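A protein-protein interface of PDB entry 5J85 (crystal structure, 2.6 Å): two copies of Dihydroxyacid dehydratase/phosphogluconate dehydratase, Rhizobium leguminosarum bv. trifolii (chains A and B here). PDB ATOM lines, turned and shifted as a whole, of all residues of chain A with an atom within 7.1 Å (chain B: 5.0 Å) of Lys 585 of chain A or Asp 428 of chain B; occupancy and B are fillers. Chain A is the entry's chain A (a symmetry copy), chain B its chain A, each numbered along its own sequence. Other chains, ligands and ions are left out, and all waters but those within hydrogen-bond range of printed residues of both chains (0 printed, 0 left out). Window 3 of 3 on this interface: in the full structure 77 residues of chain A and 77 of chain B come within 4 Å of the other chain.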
ATOM      1  N   TRP A  25     -10.135  10.110 -22.827  1.00  0.00           N
ATOM      2  CA  TRP A  25      -9.721  11.470 -23.148  1.00  0.00           C
ATOM      3  C   TRP A  25     -10.779  12.233 -23.926  1.00  0.00           C
ATOM      4  O   TRP A  25     -11.011  13.414 -23.653  1.00  0.00           O
ATOM      5  CB  TRP A  25      -8.439  11.463 -23.987  1.00  0.00           C
ATOM      6  CG  TRP A  25      -7.173  11.239 -23.244  1.00  0.00           C
ATOM      7  CD1 TRP A  25      -6.324  12.191 -22.773  1.00  0.00           C
ATOM      8  CD2 TRP A  25      -6.586   9.974 -22.915  1.00  0.00           C
ATOM      9  NE1 TRP A  25      -5.252  11.602 -22.147  1.00  0.00           N
ATOM     10  CE2 TRP A  25      -5.381  10.241 -22.229  1.00  0.00           C
ATOM     11  CE3 TRP A  25      -6.964   8.642 -23.133  1.00  0.00           C
ATOM     12  CZ2 TRP A  25      -4.543   9.225 -21.761  1.00  0.00           C
ATOM     13  CZ3 TRP A  25      -6.132   7.629 -22.665  1.00  0.00           C
ATOM     14  CH2 TRP A  25      -4.935   7.929 -21.983  1.00  0.00           C
ATOM     15  N   ALA A 582      -3.591   0.508 -18.667  1.00  0.00           N
ATOM     16  CA  ALA A 582      -4.625   1.187 -17.901  1.00  0.00           C
ATOM     17  C   ALA A 582      -4.418   2.694 -17.979  1.00  0.00           C
ATOM     18  O   ALA A 582      -3.291   3.188 -17.879  1.00  0.00           O
ATOM     19  CB  ALA A 582      -4.613   0.724 -16.446  1.00  0.00           C
ATOM     20  N   VAL A 583      -5.515   3.423 -18.186  1.00  0.00           N
ATOM     21  CA  VAL A 583      -5.448   4.879 -18.208  1.00  0.00           C
ATOM     22  C   VAL A 583      -5.094   5.388 -16.816  1.00  0.00           C
ATOM     23  O   VAL A 583      -5.659   4.944 -15.807  1.00  0.00           O
ATOM     24  CB  VAL A 583      -6.772   5.474 -18.712  1.00  0.00           C
ATOM     25  CG1 VAL A 583      -6.748   6.982 -18.609  1.00  0.00           C
ATOM     26  CG2 VAL A 583      -7.015   5.053 -20.148  1.00  0.00           C
ATOM     27  N   GLY A 584      -4.132   6.300 -16.754  1.00  0.00           N
ATOM     28  CA  GLY A 584      -3.729   6.868 -15.487  1.00  0.00           C
ATOM     29  C   GLY A 584      -4.750   7.856 -14.965  1.00  0.00           C
ATOM     30  O   GLY A 584      -5.742   8.185 -15.621  1.00  0.00           O
ATOM     31  N   LYS A 585      -4.493   8.330 -13.746  1.00  0.00           N
ATOM     32  CA  LYS A 585      -5.345   9.344 -13.141  1.00  0.00           C
ATOM     33  C   LYS A 585      -5.416  10.577 -14.039  1.00  0.00           C
ATOM     34  O   LYS A 585      -4.555  10.812 -14.889  1.00  0.00           O
ATOM     35  CB  LYS A 585      -4.832   9.721 -11.746  1.00  0.00           C
ATOM     36  CG  LYS A 585      -5.574   9.040 -10.604  1.00  0.00           C
ATOM     37  CD  LYS A 585      -4.878   9.232  -9.259  1.00  0.00           C
ATOM     38  CE  LYS A 585      -5.616   8.462  -8.158  1.00  0.00           C
ATOM     39  NZ  LYS A 585      -4.700   7.765  -7.213  1.00  0.00           N
ATOM     40  N   ASP A 586      -6.468  11.363 -13.859  1.00  0.00           N
ATOM     41  CA  ASP A 586      -6.644  12.555 -14.672  1.00  0.00           C
ATOM     42  C   ASP A 586      -5.774  13.691 -14.143  1.00  0.00           C
ATOM     43  O   ASP A 586      -5.590  13.842 -12.932  1.00  0.00           O
ATOM     44  CB  ASP A 586      -8.116  12.959 -14.697  1.00  0.00           C
ATOM     45  CG  ASP A 586      -8.609  13.240 -16.101  1.00  0.00           C
ATOM     46  OD1 ASP A 586      -7.799  13.729 -16.928  1.00  0.00           O
ATOM     47  OD2 ASP A 586      -9.796  12.944 -16.384  1.00  0.00           O
ATOM     48  N   SER A 587      -5.224  14.488 -15.063  1.00  0.00           N
ATOM     49  CA  SER A 587      -4.254  15.511 -14.688  1.00  0.00           C
ATOM     50  C   SER A 587      -4.886  16.750 -14.060  1.00  0.00           C
ATOM     51  O   SER A 587      -4.149  17.649 -13.639  1.00  0.00           O
ATOM     52  CB  SER A 587      -3.406  15.913 -15.905  1.00  0.00           C
ATOM     53  OG  SER A 587      -4.204  16.173 -17.048  1.00  0.00           O
ATOM     54  N   HIS A 588      -6.214  16.823 -13.991  1.00  0.00           N
ATOM     55  CA  HIS A 588      -6.888  17.910 -13.275  1.00  0.00           C
ATOM     56  C   HIS A 588      -8.089  17.388 -12.475  1.00  0.00           C
ATOM     57  O   HIS A 588      -8.302  16.176 -12.334  1.00  0.00           O
ATOM     58  CB  HIS A 588      -7.339  19.040 -14.232  1.00  0.00           C
ATOM     59  CG  HIS A 588      -7.946  18.566 -15.522  1.00  0.00           C
ATOM     60  ND1 HIS A 588      -7.223  17.913 -16.501  1.00  0.00           N
ATOM     61  CD2 HIS A 588      -9.214  18.659 -15.995  1.00  0.00           C
ATOM     62  CE1 HIS A 588      -8.018  17.627 -17.517  1.00  0.00           C
ATOM     63  NE2 HIS A 588      -9.231  18.068 -17.236  1.00  0.00           N
ATOM     64  OXT HIS A 588      -8.864  18.179 -11.931  1.00  0.00           O
ATOM     65  N   ARG B 104      -1.354  11.646 -19.104  1.00  0.00           N
ATOM     66  CA  ARG B 104      -1.835  11.216 -17.809  1.00  0.00           C
ATOM     67  C   ARG B 104      -0.801  10.308 -17.151  1.00  0.00           C
ATOM     68  O   ARG B 104      -0.177   9.496 -17.839  1.00  0.00           O
ATOM     69  CB  ARG B 104      -3.163  10.466 -17.948  1.00  0.00           C
ATOM     70  CG  ARG B 104      -4.252  11.247 -18.649  1.00  0.00           C
ATOM     71  CD  ARG B 104      -5.550  11.018 -17.921  1.00  0.00           C
ATOM     72  NE  ARG B 104      -6.721  11.247 -18.753  1.00  0.00           N
ATOM     73  CZ  ARG B 104      -7.917  10.739 -18.483  1.00  0.00           C
ATOM     74  NH1 ARG B 104      -8.078   9.976 -17.404  1.00  0.00           N
ATOM     75  NH2 ARG B 104      -8.944  10.997 -19.285  1.00  0.00           N
ATOM     76  N   PRO B 105      -0.618  10.381 -15.824  1.00  0.00           N
ATOM     77  CA  PRO B 105      -1.351  11.154 -14.809  1.00  0.00           C
ATOM     78  C   PRO B 105      -1.167  12.674 -14.869  1.00  0.00           C
ATOM     79  O   PRO B 105      -2.098  13.388 -14.506  1.00  0.00           O
ATOM     80  CB  PRO B 105      -0.797  10.605 -13.489  1.00  0.00           C
ATOM     81  CG  PRO B 105       0.527  10.006 -13.845  1.00  0.00           C
ATOM     82  CD  PRO B 105       0.349   9.452 -15.216  1.00  0.00           C
ATOM     83  N   ASP B 426      -6.512  12.380  -0.023  1.00  0.00           N
ATOM     84  CA  ASP B 426      -5.913  12.412  -1.358  1.00  0.00           C
ATOM     85  C   ASP B 426      -6.941  12.997  -2.318  1.00  0.00           C
ATOM     86  O   ASP B 426      -7.993  13.494  -1.898  1.00  0.00           O
ATOM     87  CB  ASP B 426      -5.426  11.030  -1.809  1.00  0.00           C
ATOM     88  CG  ASP B 426      -6.519   9.972  -1.783  1.00  0.00           C
ATOM     89  OD1 ASP B 426      -7.635  10.221  -2.296  1.00  0.00           O
ATOM     90  OD2 ASP B 426      -6.243   8.873  -1.254  1.00  0.00           O
ATOM     91  N   ILE B 427      -6.639  12.930  -3.617  1.00  0.00           N
ATOM     92  CA  ILE B 427      -7.495  13.575  -4.606  1.00  0.00           C
ATOM     93  C   ILE B 427      -8.839  12.864  -4.701  1.00  0.00           C
ATOM     94  O   ILE B 427      -9.873  13.502  -4.939  1.00  0.00           O
ATOM     95  CB  ILE B 427      -6.783  13.639  -5.973  1.00  0.00           C
ATOM     96  CG1 ILE B 427      -7.631  14.404  -6.993  1.00  0.00           C
ATOM     97  CG2 ILE B 427      -6.460  12.240  -6.485  1.00  0.00           C
ATOM     98  CD1 ILE B 427      -7.933  15.833  -6.585  1.00  0.00           C
ATOM     99  N   ASP B 428      -8.854  11.545  -4.511  1.00  0.00           N
ATOM    100  CA  ASP B 428     -10.118  10.819  -4.560  1.00  0.00           C
ATOM    101  C   ASP B 428     -11.000  11.194  -3.373  1.00  0.00           C
ATOM    102  O   ASP B 428     -12.194  11.473  -3.546  1.00  0.00           O
ATOM    103  CB  ASP B 428      -9.856   9.311  -4.611  1.00  0.00           C
ATOM    104  CG  ASP B 428      -9.242   8.872  -5.941  1.00  0.00           C
ATOM    105  OD1 ASP B 428      -9.571   9.480  -6.990  1.00  0.00           O
ATOM    106  OD2 ASP B 428      -8.424   7.925  -5.934  1.00  0.00           O
ATOM    107  N   ASP B 429     -10.411  11.243  -2.170  1.00  0.00           N
ATOM    108  CA  ASP B 429     -11.132  11.707  -0.984  1.00  0.00           C
ATOM    109  C   ASP B 429     -11.739  13.092  -1.195  1.00  0.00           C
ATOM    110  O   ASP B 429     -12.867  13.352  -0.763  1.00  0.00           O
ATOM    111  CB  ASP B 429     -10.194  11.711   0.221  1.00  0.00           C
ATOM    112  CG  ASP B 429     -10.925  11.522   1.531  1.00  0.00           C
ATOM    113  OD1 ASP B 429     -11.892  10.728   1.559  1.00  0.00           O
ATOM    114  OD2 ASP B 429     -10.520  12.148   2.538  1.00  0.00           O
ATOM    115  N   TYR B 430     -11.011  13.996  -1.861  1.00  0.00           N
ATOM    116  CA  TYR B 430     -11.552  15.331  -2.109  1.00  0.00           C
ATOM    117  C   TYR B 430     -12.807  15.267  -2.974  1.00  0.00           C
ATOM    118  O   TYR B 430     -13.828  15.881  -2.644  1.00  0.00           O
ATOM    119  CB  TYR B 430     -10.504  16.236  -2.770  1.00  0.00           C
ATOM    120  CG  TYR B 430     -11.115  17.489  -3.381  1.00  0.00           C
ATOM    121  CD1 TYR B 430     -11.523  18.547  -2.581  1.00  0.00           C
ATOM    122  CD2 TYR B 430     -11.318  17.594  -4.750  1.00  0.00           C
ATOM    123  CE1 TYR B 430     -12.097  19.681  -3.130  1.00  0.00           C
ATOM    124  CE2 TYR B 430     -11.894  18.722  -5.306  1.00  0.00           C
ATOM    125  CZ  TYR B 430     -12.283  19.763  -4.491  1.00  0.00           C
ATOM    126  OH  TYR B 430     -12.854  20.893  -5.042  1.00  0.00           O
ATOM    127  N   LYS B 431     -12.745  14.550  -4.104  1.00  0.00           N
ATOM    128  CA  LYS B 431     -13.899  14.505  -5.006  1.00  0.00           C
ATOM    129  C   LYS B 431     -15.081  13.776  -4.384  1.00  0.00           C
ATOM    130  O   LYS B 431     -16.233  14.106  -4.681  1.00  0.00           O
ATOM    131  CB  LYS B 431     -13.515  13.867  -6.349  1.00  0.00           C
ATOM    132  CG  LYS B 431     -12.157  14.311  -6.875  1.00  0.00           C
ATOM    133  CD  LYS B 431     -11.997  14.125  -8.385  1.00  0.00           C
ATOM    134  CE  LYS B 431     -11.392  12.757  -8.711  1.00  0.00           C
ATOM    135  NZ  LYS B 431     -10.481  12.785  -9.900  1.00  0.00           N
ATOM    136  N   ALA B 432     -14.820  12.804  -3.508  1.00  0.00           N
ATOM    137  CA  ALA B 432     -15.907  12.159  -2.781  1.00  0.00           C
ATOM    138  C   ALA B 432     -16.607  13.131  -1.830  1.00  0.00           C
ATOM    139  O   ALA B 432     -17.842  13.143  -1.748  1.00  0.00           O
ATOM    140  CB  ALA B 432     -15.372  10.950  -2.012  1.00  0.00           C
ATOM    141  N   TYR B 457       0.921  11.891  -6.016  1.00  0.00           N
ATOM    142  CA  TYR B 457      -0.242  11.879  -6.904  1.00  0.00           C
ATOM    143  C   TYR B 457      -0.337  10.629  -7.774  1.00  0.00           C
ATOM    144  O   TYR B 457      -1.436  10.050  -7.861  1.00  0.00           O
ATOM    145  CB  TYR B 457      -0.261  13.144  -7.759  1.00  0.00           C
ATOM    146  CG  TYR B 457      -1.571  13.323  -8.479  1.00  0.00           C
ATOM    147  CD1 TYR B 457      -2.653  13.924  -7.843  1.00  0.00           C
ATOM    148  CD2 TYR B 457      -1.743  12.869  -9.785  1.00  0.00           C
ATOM    149  CE1 TYR B 457      -3.866  14.091  -8.493  1.00  0.00           C
ATOM    150  CE2 TYR B 457      -2.956  13.028 -10.445  1.00  0.00           C
ATOM    151  CZ  TYR B 457      -4.012  13.641  -9.789  1.00  0.00           C
ATOM    152  OH  TYR B 457      -5.217  13.811 -10.419  1.00  0.00           O
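The guanidinium group (NH1) of Arg 104 of chain B lies within hydrogen-bond range of the backbone carbonyl oxygen (O) of Gly 584 of chain A, 3.4 Å away. OD1 of Asp 586 of chain A lies within salt-bridge range of NE of Arg 104 of chain B (3.3 Å). The backbone carbonyl oxygen (O) of Pro 105 of chain B lies close to the backbone NH (N) of Ser 587 of chain A, 3.4 Å away. The side-chain amino group (NZ) of Lys 585 of chain A lies within salt-bridge range of the side-chain carboxylate (OD2) of Asp 428 of chain B (3.9 Å). The side-chain hydroxyl (OH) of Tyr 457 of chain B is in hydrogen-bond range of the backbone carbonyl oxygen (O) of Asp 586 of chain A (2.5 Å).
Arg 104 of chain B touches Trp 25 of chain A (CG to NE1, 3.7 Å). Val 583 of chain A touches Arg 104 of chain B. O of Lys 585 of chain A touches CD of Arg 104 of chain B, at 3.2 Å. Pro 105 of chain B touches Lys 585 of chain A. Tyr 457 of chain B touches Lys 585 of chain A (O to CD, 3.8 Å). Pro 105 of chain B touches Asp 586 of chain A.
The side-chain carboxylate of Asp 426 of chain B lies within hydrogen-bond range of the backbone NH of Asp 428 of chain B, at 2.9 Å.
No position is printed for both chains. Of the 11 pairs that touch across the chains among the printed residues, none has its exchanged pair printed and touching as well.
Printed residues of chain B within 4 Å of Trp 25 of chain A: Arg 104. Printed residues of chain B within 4 Å of Gly 584 of chain A: Arg 104. Lys 585 of chain A touches four residues of chain B. Of the printed residues of chain B, Asp 586 of chain A touches Arg 104 (3.3 Å), Pro 105 (3.7 Å) and Tyr 457 (2.5 Å). Of the printed residues of chain A, Pro 105 of chain B touches Lys 585, Asp 586 and Ser 587. Of the printed residues of chain A, Tyr 457 of chain B touches Lys 585 and Asp 586. The nearest residue of chain B that does not touch Lys 585 of chain A is Ile 427 of chain B (4.2 Å). The nearest printed residue of chain B that does not touch Ser 587 of chain A is Arg 104 of chain B (4.5 Å).
Along chain B the printed residues that touch a printed residue of chain A span positions 104 to 457. Among the printed residues, 11 pairs touch across the chains. Among the printed residues, Asp or Glu carboxylates within 4 Å of a Lys or Arg side-chain nitrogen of the other chain: Lys 585 of chain A with Asp 428 of chain B and Asp 586 of chain A with Arg 104 of chain B.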
